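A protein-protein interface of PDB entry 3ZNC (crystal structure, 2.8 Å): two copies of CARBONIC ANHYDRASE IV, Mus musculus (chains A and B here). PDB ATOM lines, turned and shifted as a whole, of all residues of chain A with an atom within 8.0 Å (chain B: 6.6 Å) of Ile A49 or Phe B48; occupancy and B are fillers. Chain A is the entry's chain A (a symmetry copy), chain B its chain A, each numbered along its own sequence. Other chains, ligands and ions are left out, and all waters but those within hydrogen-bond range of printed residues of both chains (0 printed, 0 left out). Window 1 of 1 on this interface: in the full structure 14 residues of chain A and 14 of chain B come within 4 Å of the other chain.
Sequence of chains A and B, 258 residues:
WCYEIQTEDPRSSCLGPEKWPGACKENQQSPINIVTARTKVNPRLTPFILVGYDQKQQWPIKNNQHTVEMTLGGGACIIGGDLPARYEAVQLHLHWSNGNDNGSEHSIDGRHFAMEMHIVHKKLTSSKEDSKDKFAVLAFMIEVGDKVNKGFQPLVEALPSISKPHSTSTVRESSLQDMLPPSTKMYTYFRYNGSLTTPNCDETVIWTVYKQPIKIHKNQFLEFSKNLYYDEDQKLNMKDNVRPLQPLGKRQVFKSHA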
ATOM      1  N   THR A  46      -9.391 -11.687  -7.617  1.00  0.00           N
ATOM      2  CA  THR A  46      -8.563 -12.849  -7.882  1.00  0.00           C
ATOM      3  C   THR A  46      -8.839 -13.197  -9.349  1.00  0.00           C
ATOM      4  O   THR A  46      -9.944 -12.955  -9.839  1.00  0.00           O
ATOM      5  CB  THR A  46      -8.943 -13.988  -6.885  1.00  0.00           C
ATOM      6  OG1 THR A  46      -8.173 -15.159  -7.155  1.00  0.00           O
ATOM      7  CG2 THR A  46     -10.429 -14.320  -6.950  1.00  0.00           C
ATOM      8  N   PRO A  47      -7.831 -13.715 -10.083  1.00  0.00           N
ATOM      9  CA  PRO A  47      -7.996 -14.075 -11.504  1.00  0.00           C
ATOM     10  C   PRO A  47      -9.215 -14.932 -11.870  1.00  0.00           C
ATOM     11  O   PRO A  47      -9.661 -15.779 -11.093  1.00  0.00           O
ATOM     12  CB  PRO A  47      -6.626 -14.759 -11.865  1.00  0.00           C
ATOM     13  CG  PRO A  47      -6.083 -15.171 -10.530  1.00  0.00           C
ATOM     14  CD  PRO A  47      -6.463 -14.021  -9.631  1.00  0.00           C
ATOM     15  N   PHE A  48      -9.763 -14.677 -13.054  1.00  0.00           N
ATOM     16  CA  PHE A  48     -10.937 -15.390 -13.540  1.00  0.00           C
ATOM     17  C   PHE A  48     -10.692 -16.855 -13.835  1.00  0.00           C
ATOM     18  O   PHE A  48      -9.577 -17.261 -14.163  1.00  0.00           O
ATOM     19  CB  PHE A  48     -11.499 -14.710 -14.847  1.00  0.00           C
ATOM     20  CG  PHE A  48     -12.306 -13.472 -14.596  1.00  0.00           C
ATOM     21  CD1 PHE A  48     -13.503 -13.539 -13.896  1.00  0.00           C
ATOM     22  CD2 PHE A  48     -11.876 -12.235 -15.070  1.00  0.00           C
ATOM     23  CE1 PHE A  48     -14.258 -12.392 -13.671  1.00  0.00           C
ATOM     24  CE2 PHE A  48     -12.626 -11.085 -14.850  1.00  0.00           C
ATOM     25  CZ  PHE A  48     -13.818 -11.164 -14.149  1.00  0.00           C
ATOM     26  N   ILE A  49     -11.746 -17.648 -13.687  1.00  0.00           N
ATOM     27  CA  ILE A  49     -11.701 -19.068 -13.995  1.00  0.00           C
ATOM     28  C   ILE A  49     -12.269 -19.059 -15.405  1.00  0.00           C
ATOM     29  O   ILE A  49     -13.447 -18.734 -15.600  1.00  0.00           O
ATOM     30  CB  ILE A  49     -12.649 -19.876 -13.100  1.00  0.00           C
ATOM     31  CG1 ILE A  49     -12.429 -19.503 -11.594  1.00  0.00           C
ATOM     32  CG2 ILE A  49     -12.432 -21.360 -13.326  1.00  0.00           C
ATOM     33  CD1 ILE A  49     -13.572 -19.903 -10.695  1.00  0.00           C
ATOM     34  N   LEU A  50     -11.415 -19.309 -16.393  1.00  0.00           N
ATOM     35  CA  LEU A  50     -11.843 -19.294 -17.786  1.00  0.00           C
ATOM     36  C   LEU A  50     -12.329 -20.649 -18.273  1.00  0.00           C
ATOM     37  O   LEU A  50     -11.539 -21.567 -18.490  1.00  0.00           O
ATOM     38  CB  LEU A  50     -10.689 -18.762 -18.696  1.00  0.00           C
ATOM     39  CG  LEU A  50     -10.214 -17.302 -18.393  1.00  0.00           C
ATOM     40  CD1 LEU A  50      -9.057 -16.948 -19.316  1.00  0.00           C
ATOM     41  CD2 LEU A  50     -11.370 -16.315 -18.567  1.00  0.00           C
ATOM     42  N   VAL A  51     -13.639 -20.759 -18.462  1.00  0.00           N
ATOM     43  CA  VAL A  51     -14.248 -21.995 -18.922  1.00  0.00           C
ATOM     44  C   VAL A  51     -14.575 -21.907 -20.409  1.00  0.00           C
ATOM     45  O   VAL A  51     -15.074 -20.885 -20.884  1.00  0.00           O
ATOM     46  CB  VAL A  51     -15.537 -22.315 -18.132  1.00  0.00           C
ATOM     47  CG1 VAL A  51     -16.253 -23.510 -18.741  1.00  0.00           C
ATOM     48  CG2 VAL A  51     -15.203 -22.592 -16.680  1.00  0.00           C
ATOM     49  N   GLY A  52     -14.275 -22.978 -21.138  1.00  0.00           N
ATOM     50  CA  GLY A  52     -14.558 -23.014 -22.561  1.00  0.00           C
ATOM     51  C   GLY A  52     -13.610 -22.192 -23.423  1.00  0.00           C
ATOM     52  O   GLY A  52     -13.814 -22.093 -24.637  1.00  0.00           O
ATOM     53  N   TYR A  53     -12.580 -21.604 -22.815  1.00  0.00           N
ATOM     54  CA  TYR A  53     -11.613 -20.802 -23.564  1.00  0.00           C
ATOM     55  C   TYR A  53     -10.601 -21.684 -24.279  1.00  0.00           C
ATOM     56  O   TYR A  53      -9.942 -21.244 -25.219  1.00  0.00           O
ATOM     57  CB  TYR A  53     -10.866 -19.782 -22.619  1.00  0.00           C
ATOM     58  CG  TYR A  53     -11.615 -18.487 -22.412  1.00  0.00           C
ATOM     59  CD1 TYR A  53     -12.901 -18.483 -21.861  1.00  0.00           C
ATOM     60  CD2 TYR A  53     -11.054 -17.265 -22.800  1.00  0.00           C
ATOM     61  CE1 TYR A  53     -13.612 -17.299 -21.702  1.00  0.00           C
ATOM     62  CE2 TYR A  53     -11.754 -16.072 -22.648  1.00  0.00           C
ATOM     63  CZ  TYR A  53     -13.035 -16.094 -22.098  1.00  0.00           C
ATOM     64  OH  TYR A  53     -13.740 -14.916 -21.949  1.00  0.00           O
ATOM     65  N   ALA A  76     -18.254 -20.239 -24.220  1.00  0.00           N
ATOM     66  CA  ALA A  76     -17.373 -20.010 -23.074  1.00  0.00           C
ATOM     67  C   ALA A  76     -18.150 -19.438 -21.896  1.00  0.00           C
ATOM     68  O   ALA A  76     -19.232 -18.884 -22.076  1.00  0.00           O
ATOM     69  CB  ALA A  76     -16.250 -19.081 -23.457  1.00  0.00           C
ATOM     70  N   CYS A  77     -17.554 -19.497 -20.711  1.00  0.00           N
ATOM     71  CA  CYS A  77     -18.192 -19.020 -19.481  1.00  0.00           C
ATOM     72  C   CYS A  77     -17.062 -18.534 -18.577  1.00  0.00           C
ATOM     73  O   CYS A  77     -15.923 -18.979 -18.733  1.00  0.00           O
ATOM     74  CB  CYS A  77     -18.959 -20.237 -18.799  1.00  0.00           C
ATOM     75  SG  CYS A  77     -20.250 -19.888 -17.541  1.00  0.00           S
ATOM     76  N   ILE A  78     -17.339 -17.575 -17.700  1.00  0.00           N
ATOM     77  CA  ILE A  78     -16.320 -17.083 -16.774  1.00  0.00           C
ATOM     78  C   ILE A  78     -16.908 -17.049 -15.374  1.00  0.00           C
ATOM     79  O   ILE A  78     -18.085 -16.726 -15.186  1.00  0.00           O
ATOM     80  CB  ILE A  78     -15.783 -15.677 -17.127  1.00  0.00           C
ATOM     81  CG1 ILE A  78     -16.942 -14.634 -17.192  1.00  0.00           C
ATOM     82  CG2 ILE A  78     -15.000 -15.719 -18.419  1.00  0.00           C
ATOM     83  CD1 ILE A  78     -16.444 -13.215 -17.187  1.00  0.00           C
ATOM     84  N   ILE A  79     -16.089 -17.391 -14.391  1.00  0.00           N
ATOM     85  CA  ILE A  79     -16.535 -17.423 -13.012  1.00  0.00           C
ATOM     86  C   ILE A  79     -15.494 -16.724 -12.150  1.00  0.00           C
ATOM     87  O   ILE A  79     -14.314 -16.680 -12.508  1.00  0.00           O
ATOM     88  CB  ILE A  79     -16.666 -18.889 -12.537  1.00  0.00           C
ATOM     89  CG1 ILE A  79     -17.483 -19.724 -13.590  1.00  0.00           C
ATOM     90  CG2 ILE A  79     -17.352 -18.950 -11.186  1.00  0.00           C
ATOM     91  CD1 ILE A  79     -17.199 -21.200 -13.565  1.00  0.00           C
ATOM     92  N   GLY A  80     -15.929 -16.144 -11.038  1.00  0.00           N
ATOM     93  CA  GLY A  80     -14.995 -15.492 -10.135  1.00  0.00           C
ATOM     94  C   GLY A  80     -14.796 -14.010 -10.339  1.00  0.00           C
ATOM     95  O   GLY A  80     -15.735 -13.301 -10.691  1.00  0.00           O
ATOM     96  N   GLY A  81     -13.581 -13.543 -10.059  1.00  0.00           N
ATOM     97  CA  GLY A  81     -13.247 -12.133 -10.202  1.00  0.00           C
ATOM     98  C   GLY A  81     -14.229 -11.233  -9.478  1.00  0.00           C
ATOM     99  O   GLY A  81     -14.583 -10.164  -9.969  1.00  0.00           O
ATOM    100  N   ARG A  86     -22.341 -15.942 -12.619  1.00  0.00           N
ATOM    101  CA  ARG A  86     -21.542 -16.490 -13.709  1.00  0.00           C
ATOM    102  C   ARG A  86     -21.975 -15.815 -15.004  1.00  0.00           C
ATOM    103  O   ARG A  86     -23.154 -15.535 -15.198  1.00  0.00           O
ATOM    104  CB  ARG A  86     -21.766 -18.030 -13.821  1.00  0.00           C
ATOM    105  CG  ARG A  86     -21.269 -18.812 -12.625  1.00  0.00           C
ATOM    106  CD  ARG A  86     -21.766 -20.253 -12.660  1.00  0.00           C
ATOM    107  NE  ARG A  86     -21.145 -21.054 -11.612  1.00  0.00           N
ATOM    108  CZ  ARG A  86     -20.735 -22.307 -11.773  1.00  0.00           C
ATOM    109  NH1 ARG A  86     -20.905 -22.922 -12.939  1.00  0.00           N
ATOM    110  NH2 ARG A  86     -20.167 -22.952 -10.761  1.00  0.00           N
ATOM    111  N   TYR A  87     -21.021 -15.529 -15.877  1.00  0.00           N
ATOM    112  CA  TYR A  87     -21.324 -14.882 -17.144  1.00  0.00           C
ATOM    113  C   TYR A  87     -20.855 -15.749 -18.303  1.00  0.00           C
ATOM    114  O   TYR A  87     -19.861 -16.471 -18.184  1.00  0.00           O
ATOM    115  CB  TYR A  87     -20.620 -13.487 -17.219  1.00  0.00           C
ATOM    116  CG  TYR A  87     -21.127 -12.487 -16.217  1.00  0.00           C
ATOM    117  CD1 TYR A  87     -20.941 -12.681 -14.855  1.00  0.00           C
ATOM    118  CD2 TYR A  87     -21.796 -11.343 -16.631  1.00  0.00           C
ATOM    119  CE1 TYR A  87     -21.414 -11.762 -13.932  1.00  0.00           C
ATOM    120  CE2 TYR A  87     -22.267 -10.421 -15.718  1.00  0.00           C
ATOM    121  CZ  TYR A  87     -22.077 -10.637 -14.376  1.00  0.00           C
ATOM    122  OH  TYR A  87     -22.566  -9.734 -13.473  1.00  0.00           O
ATOM    123  N   HIS A 121     -19.676 -10.521 -22.065  1.00  0.00           N
ATOM    124  CA  HIS A 121     -20.313 -11.627 -21.352  1.00  0.00           C
ATOM    125  C   HIS A 121     -21.653 -11.182 -20.763  1.00  0.00           C
ATOM    126  O   HIS A 121     -21.726 -10.170 -20.073  1.00  0.00           O
ATOM    127  CB  HIS A 121     -19.384 -12.138 -20.188  1.00  0.00           C
ATOM    128  CG  HIS A 121     -18.044 -12.623 -20.646  1.00  0.00           C
ATOM    129  ND1 HIS A 121     -17.654 -13.942 -20.547  1.00  0.00           N
ATOM    130  CD2 HIS A 121     -17.000 -11.966 -21.200  1.00  0.00           C
ATOM    131  CE1 HIS A 121     -16.430 -14.076 -21.023  1.00  0.00           C
ATOM    132  NE2 HIS A 121     -16.011 -12.891 -21.425  1.00  0.00           N
ATOM    133  N   TYR A 210      -7.254  -5.326 -18.529  1.00  0.00           N
ATOM    134  CA  TYR A 210      -5.979  -5.939 -18.144  1.00  0.00           C
ATOM    135  C   TYR A 210      -4.764  -5.069 -18.481  1.00  0.00           C
ATOM    136  O   TYR A 210      -4.730  -4.421 -19.526  1.00  0.00           O
ATOM    137  CB  TYR A 210      -5.826  -7.351 -18.799  1.00  0.00           C
ATOM    138  CG  TYR A 210      -6.761  -8.399 -18.242  1.00  0.00           C
ATOM    139  CD1 TYR A 210      -8.067  -8.523 -18.719  1.00  0.00           C
ATOM    140  CD2 TYR A 210      -6.325  -9.299 -17.271  1.00  0.00           C
ATOM    141  CE1 TYR A 210      -8.913  -9.526 -18.242  1.00  0.00           C
ATOM    142  CE2 TYR A 210      -7.161 -10.304 -16.790  1.00  0.00           C
ATOM    143  CZ  TYR A 210      -8.449 -10.412 -17.280  1.00  0.00           C
ATOM    144  OH  TYR A 210      -9.259 -11.412 -16.807  1.00  0.00           O
ATOM    145  N   THR B  46     -15.742 -24.343  -6.068  1.00  0.00           N
ATOM    146  CA  THR B  46     -15.811 -23.756  -7.394  1.00  0.00           C
ATOM    147  C   THR B  46     -14.508 -24.187  -8.078  1.00  0.00           C
ATOM    148  O   THR B  46     -13.491 -24.363  -7.404  1.00  0.00           O
ATOM    149  CB  THR B  46     -15.969 -22.210  -7.263  1.00  0.00           C
ATOM    150  OG1 THR B  46     -15.994 -21.604  -8.555  1.00  0.00           O
ATOM    151  CG2 THR B  46     -14.851 -21.598  -6.426  1.00  0.00           C
ATOM    152  N   PRO B  47     -14.532 -24.416  -9.409  1.00  0.00           N
ATOM    153  CA  PRO B  47     -13.333 -24.840 -10.155  1.00  0.00           C
ATOM    154  C   PRO B  47     -12.047 -24.033  -9.928  1.00  0.00           C
ATOM    155  O   PRO B  47     -12.081 -22.823  -9.699  1.00  0.00           O
ATOM    156  CB  PRO B  47     -13.815 -24.828 -11.652  1.00  0.00           C
ATOM    157  CG  PRO B  47     -15.010 -23.922 -11.623  1.00  0.00           C
ATOM    158  CD  PRO B  47     -15.681 -24.276 -10.319  1.00  0.00           C
ATOM    159  N   PHE B  48     -10.916 -24.731  -9.967  1.00  0.00           N
ATOM    160  CA  PHE B  48      -9.613 -24.116  -9.751  1.00  0.00           C
ATOM    161  C   PHE B  48      -9.196 -23.152 -10.843  1.00  0.00           C
ATOM    162  O   PHE B  48      -9.604 -23.282 -11.997  1.00  0.00           O
ATOM    163  CB  PHE B  48      -8.494 -25.218  -9.612  1.00  0.00           C
ATOM    164  CG  PHE B  48      -8.448 -25.879  -8.267  1.00  0.00           C
ATOM    165  CD1 PHE B  48      -8.127 -25.147  -7.131  1.00  0.00           C
ATOM    166  CD2 PHE B  48      -8.715 -27.239  -8.134  1.00  0.00           C
ATOM    167  CE1 PHE B  48      -8.074 -25.762  -5.884  1.00  0.00           C
ATOM    168  CE2 PHE B  48      -8.663 -27.860  -6.890  1.00  0.00           C
ATOM    169  CZ  PHE B  48      -8.343 -27.120  -5.764  1.00  0.00           C
ATOM    170  N   ILE B  49      -8.398 -22.166 -10.455  1.00  0.00           N
ATOM    171  CA  ILE B  49      -7.850 -21.194 -11.389  1.00  0.00           C
ATOM    172  C   ILE B  49      -6.485 -21.809 -11.650  1.00  0.00           C
ATOM    173  O   ILE B  49      -5.647 -21.875 -10.742  1.00  0.00           O
ATOM    174  CB  ILE B  49      -7.644 -19.824 -10.730  1.00  0.00           C
ATOM    175  CG1 ILE B  49      -8.942 -19.379  -9.976  1.00  0.00           C
ATOM    176  CG2 ILE B  49      -7.252 -18.802 -11.780  1.00  0.00           C
ATOM    177  CD1 ILE B  49      -8.712 -18.287  -8.961  1.00  0.00           C
ATOM    178  N   LEU B  50      -6.295 -22.350 -12.850  1.00  0.00           N
ATOM    179  CA  LEU B  50      -5.036 -22.995 -13.199  1.00  0.00           C
ATOM    180  C   LEU B  50      -4.026 -22.037 -13.810  1.00  0.00           C
ATOM    181  O   LEU B  50      -4.166 -21.612 -14.956  1.00  0.00           O
ATOM    182  CB  LEU B  50      -5.299 -24.202 -14.156  1.00  0.00           C
ATOM    183  CG  LEU B  50      -6.199 -25.341 -13.569  1.00  0.00           C
ATOM    184  CD1 LEU B  50      -6.410 -26.412 -14.629  1.00  0.00           C
ATOM    185  CD2 LEU B  50      -5.559 -25.936 -12.314  1.00  0.00           C
ATOM    186  N   ILE B  78      -1.879 -22.940  -8.383  1.00  0.00           N
ATOM    187  CA  ILE B  78      -3.332 -23.103  -8.399  1.00  0.00           C
ATOM    188  C   ILE B  78      -3.933 -22.236  -7.307  1.00  0.00           C
ATOM    189  O   ILE B  78      -3.364 -22.097  -6.219  1.00  0.00           O
ATOM    190  CB  ILE B  78      -3.799 -24.563  -8.194  1.00  0.00           C
ATOM    191  CG1 ILE B  78      -3.247 -25.145  -6.855  1.00  0.00           C
ATOM    192  CG2 ILE B  78      -3.401 -25.416  -9.376  1.00  0.00           C
ATOM    193  CD1 ILE B  78      -3.943 -26.414  -6.447  1.00  0.00           C
ATOM    194  N   ILE B  79      -5.081 -21.644  -7.600  1.00  0.00           N
ATOM    195  CA  ILE B  79      -5.745 -20.771  -6.653  1.00  0.00           C
ATOM    196  C   ILE B  79      -7.220 -21.141  -6.605  1.00  0.00           C
ATOM    197  O   ILE B  79      -7.764 -21.667  -7.579  1.00  0.00           O
ATOM    198  CB  ILE B  79      -5.618 -19.301  -7.117  1.00  0.00           C
ATOM    199  CG1 ILE B  79      -4.124 -18.980  -7.486  1.00  0.00           C
ATOM    200  CG2 ILE B  79      -6.096 -18.358  -6.030  1.00  0.00           C
ATOM    201  CD1 ILE B  79      -3.955 -17.848  -8.459  1.00  0.00           C
ATOM    202  N   GLY B  80      -7.860 -20.906  -5.465  1.00  0.00           N
ATOM    203  CA  GLY B  80      -9.280 -21.188  -5.347  1.00  0.00           C
ATOM    204  C   GLY B  80      -9.646 -22.544  -4.794  1.00  0.00           C
ATOM    205  O   GLY B  80      -8.954 -23.066  -3.924  1.00  0.00           O
ATOM    206  N   GLY B  81     -10.769 -23.080  -5.267  1.00  0.00           N
ATOM    207  CA  GLY B  81     -11.249 -24.380  -4.818  1.00  0.00           C
ATOM    208  C   GLY B  81     -11.333 -24.471  -3.306  1.00  0.00           C
ATOM    209  O   GLY B  81     -11.024 -25.506  -2.720  1.00  0.00           O
ATOM    210  N   ASP B  82     -11.761 -23.380  -2.681  1.00  0.00           N
ATOM    211  CA  ASP B  82     -11.875 -23.296  -1.228  1.00  0.00           C
ATOM    212  C   ASP B  82     -10.605 -23.735  -0.482  1.00  0.00           C
ATOM    213  O   ASP B  82     -10.668 -24.235   0.647  1.00  0.00           O
ATOM    214  CB  ASP B  82     -13.146 -24.067  -0.694  1.00  0.00           C
ATOM    215  CG  ASP B  82     -13.587 -23.583   0.693  1.00  0.00           C
ATOM    216  OD1 ASP B  82     -13.463 -22.366   0.972  1.00  0.00           O
ATOM    217  OD2 ASP B  82     -14.057 -24.416   1.502  1.00  0.00           O
ATOM    218  N   LEU B  83      -9.459 -23.570  -1.134  1.00  0.00           N
ATOM    219  CA  LEU B  83      -8.171 -23.888  -0.525  1.00  0.00           C
ATOM    220  C   LEU B  83      -7.848 -22.695   0.377  1.00  0.00           C
ATOM    221  O   LEU B  83      -8.302 -21.577   0.123  1.00  0.00           O
ATOM    222  CB  LEU B  83      -7.069 -24.059  -1.630  1.00  0.00           C
ATOM    223  CG  LEU B  83      -6.607 -25.523  -1.986  1.00  0.00           C
ATOM    224  CD1 LEU B  83      -7.767 -26.488  -2.012  1.00  0.00           C
ATOM    225  CD2 LEU B  83      -5.886 -25.517  -3.317  1.00  0.00           C
ATOM    226  N   ALA B 136      -1.739 -30.079  -1.630  1.00  0.00           N
ATOM    227  CA  ALA B 136      -2.993 -30.095  -2.354  1.00  0.00           C
ATOM    228  C   ALA B 136      -2.679 -31.026  -3.511  1.00  0.00           C
ATOM    229  O   ALA B 136      -1.846 -30.714  -4.370  1.00  0.00           O
ATOM    230  CB  ALA B 136      -3.348 -28.706  -2.851  1.00  0.00           C
ATOM    231  N   LEU B 138      -4.070 -33.119  -6.677  1.00  0.00           N
ATOM    232  CA  LEU B 138      -5.156 -33.276  -7.629  1.00  0.00           C
ATOM    233  C   LEU B 138      -5.007 -34.681  -8.221  1.00  0.00           C
ATOM    234  O   LEU B 138      -3.939 -35.048  -8.722  1.00  0.00           O
ATOM    235  CB  LEU B 138      -5.068 -32.199  -8.754  1.00  0.00           C
ATOM    236  CG  LEU B 138      -4.900 -30.723  -8.266  1.00  0.00           C
ATOM    237  CD1 LEU B 138      -4.973 -29.802  -9.480  1.00  0.00           C
ATOM    238  CD2 LEU B 138      -5.970 -30.364  -7.247  1.00  0.00           C
ATOM    239  N   MET B 186     -14.073 -30.181 -15.897  1.00  0.00           N
ATOM    240  CA  MET B 186     -13.441 -30.108 -14.590  1.00  0.00           C
ATOM    241  C   MET B 186     -14.295 -29.407 -13.550  1.00  0.00           C
ATOM    242  O   MET B 186     -13.785 -28.822 -12.593  1.00  0.00           O
ATOM    243  CB  MET B 186     -12.034 -29.442 -14.708  1.00  0.00           C
ATOM    244  CG  MET B 186     -11.066 -30.256 -15.544  1.00  0.00           C
ATOM    245  SD  MET B 186      -9.373 -29.840 -15.171  1.00  0.00           S
ATOM    246  CE  MET B 186      -9.104 -28.506 -16.326  1.00  0.00           C
ATOM    247  N   TYR B 189     -15.933 -32.694  -9.015  1.00  0.00           N
ATOM    248  CA  TYR B 189     -14.854 -33.349  -8.290  1.00  0.00           C
ATOM    249  C   TYR B 189     -15.229 -33.611  -6.834  1.00  0.00           C
ATOM    250  O   TYR B 189     -16.317 -33.233  -6.392  1.00  0.00           O
ATOM    251  CB  TYR B 189     -13.513 -32.526  -8.394  1.00  0.00           C
ATOM    252  CG  TYR B 189     -13.563 -31.097  -7.887  1.00  0.00           C
ATOM    253  CD1 TYR B 189     -13.397 -30.811  -6.535  1.00  0.00           C
ATOM    254  CD2 TYR B 189     -13.703 -30.030  -8.771  1.00  0.00           C
ATOM    255  CE1 TYR B 189     -13.358 -29.503  -6.078  1.00  0.00           C
ATOM    256  CE2 TYR B 189     -13.666 -28.717  -8.326  1.00  0.00           C
ATOM    257  CZ  TYR B 189     -13.491 -28.459  -6.976  1.00  0.00           C
ATOM    258  OH  TYR B 189     -13.433 -27.157  -6.517  1.00  0.00           O
ATOM    259  N   ARG B 191     -13.798 -33.582  -2.623  1.00  0.00           N
ATOM    260  CA  ARG B 191     -12.826 -33.060  -1.677  1.00  0.00           C
ATOM    261  C   ARG B 191     -12.890 -33.831  -0.371  1.00  0.00           C
ATOM    262  O   ARG B 191     -13.957 -34.306   0.018  1.00  0.00           O
ATOM    263  CB  ARG B 191     -13.117 -31.540  -1.405  1.00  0.00           C
ATOM    264  CG  ARG B 191     -12.227 -30.880  -0.365  1.00  0.00           C
ATOM    265  CD  ARG B 191     -10.769 -30.819  -0.804  1.00  0.00           C
ATOM    266  NE  ARG B 191     -10.567 -30.080  -2.049  1.00  0.00           N
ATOM    267  CZ  ARG B 191     -10.851 -28.794  -2.219  1.00  0.00           C
ATOM    268  NH1 ARG B 191     -11.351 -28.080  -1.220  1.00  0.00           N
ATOM    269  NH2 ARG B 191     -10.655 -28.225  -3.399  1.00  0.00           N
ATOM    270  N   THR B 208      -8.337 -33.689  -3.946  1.00  0.00           N
ATOM    271  CA  THR B 208      -9.343 -33.284  -4.919  1.00  0.00           C
ATOM    272  C   THR B 208      -9.289 -34.357  -6.005  1.00  0.00           C
ATOM    273  O   THR B 208      -8.289 -34.494  -6.705  1.00  0.00           O
ATOM    274  CB  THR B 208      -9.034 -31.898  -5.519  1.00  0.00           C
ATOM    275  OG1 THR B 208      -9.082 -30.905  -4.489  1.00  0.00           O
ATOM    276  CG2 THR B 208     -10.041 -31.541  -6.592  1.00  0.00           C
ATOM    277  N   TYR B 210     -11.115 -35.833  -9.333  1.00  0.00           N
ATOM    278  CA  TYR B 210     -12.078 -35.457 -10.374  1.00  0.00           C
ATOM    279  C   TYR B 210     -12.869 -36.648 -10.923  1.00  0.00           C
ATOM    280  O   TYR B 210     -12.323 -37.736 -11.095  1.00  0.00           O
ATOM    281  CB  TYR B 210     -11.360 -34.705 -11.543  1.00  0.00           C
ATOM    282  CG  TYR B 210     -10.863 -33.326 -11.181  1.00  0.00           C
ATOM    283  CD1 TYR B 210      -9.628 -33.147 -10.555  1.00  0.00           C
ATOM    284  CD2 TYR B 210     -11.606 -32.192 -11.509  1.00  0.00           C
ATOM    285  CE1 TYR B 210      -9.146 -31.869 -10.270  1.00  0.00           C
ATOM    286  CE2 TYR B 210     -11.133 -30.912 -11.229  1.00  0.00           C
ATOM    287  CZ  TYR B 210      -9.905 -30.758 -10.613  1.00  0.00           C
ATOM    288  OH  TYR B 210      -9.444 -29.494 -10.353  1.00  0.00           O
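Of the 18 printed residues of chain B, 5 touch a printed residue of chain A. Hydrophobic or aromatic side chains of chain B that line the printed part of chain A: Pro B47, Ile B49 and Ile B79. Among the printed residues, no Asp or Glu carboxylate lies within 4 Å of a Lys or Arg side-chain nitrogen of the other chain.
Thr A46 touches Ile B49 (OG1 to CD1, 3.7 Å). OG1 of Thr A46 touches CG2 of Ile B79 (3.98 Å). O of Pro A47 touches CD1 of Ile B49 (3.4 Å). Pro A47 touches Ile B79 (CG to CD1, 3.998 Å). O of Phe A48 touches CG2 of Ile B49 (3.7 Å). Ile A49 touches Thr B46. O of Pro B47 touches CD1 of Ile A49, at 3.4 Å. Phe B48 touches Ile A49. Ile B49 touches Ile A49 (CG1 to CG1, 3.8 Å). CD1 of Ile A79 touches CG of Pro B47 (3.997 Å).
The backbone NH (N) of Ile A49 sits at hydrogen-bond distance from the backbone carbonyl oxygen (O) of Ile A79, at 3.0 Å. OH of Tyr B189 lies within hydrogen-bond range of O of Thr B46 (2.9 Å). The backbone carbonyl oxygen of Ile B79 lies within hydrogen-bond range of the backbone NH of Ile B49, at 3.0 Å.
Printed residues of chain B within 4 Å of Ile A49: Thr B46 (3.7 Å), Pro B47 (3.4 Å), Phe B48 (3.7 Å) and Ile B49 (3.8 Å). Printed residues of chain B within 4 Å of Pro A47: Ile B49 and Ile B79. Of the printed residues of chain B, Ile A79 touches Thr B46 (3.98 Å) and Pro B47 (3.997 Å). Of the printed residues of chain A, Ile B79 touches Thr A46 (3.98 Å) and Pro A47 (3.998 Å). Of the printed residues of chain A, Ile B49 touches Thr A46, Pro A47, Phe A48 and Ile A49. Of the printed residues of chain B, Phe A48 touches Ile B49. The nearest residue of chain B that does not touch Ile A49 is Leu B50 (6.2 Å). The nearest printed residue of chain A that does not touch Ile B49 is Leu A50 (6.2 Å).
Thr A46 touches Ile B49, and with the chains exchanged Ile A49 touches Thr B46. Pro A47 touches Ile B49, and with the chains exchanged Ile A49 touches Pro B47. Pro A47 touches Ile B79, and with the chains exchanged Ile A79 touches Pro B47. Phe A48 touches Ile B49, and with the chains exchanged Ile A49 touches Phe B48. Of the 11 pairs that touch across the chains among the printed residues, 11 have their exchanged pair printed and touching as well.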
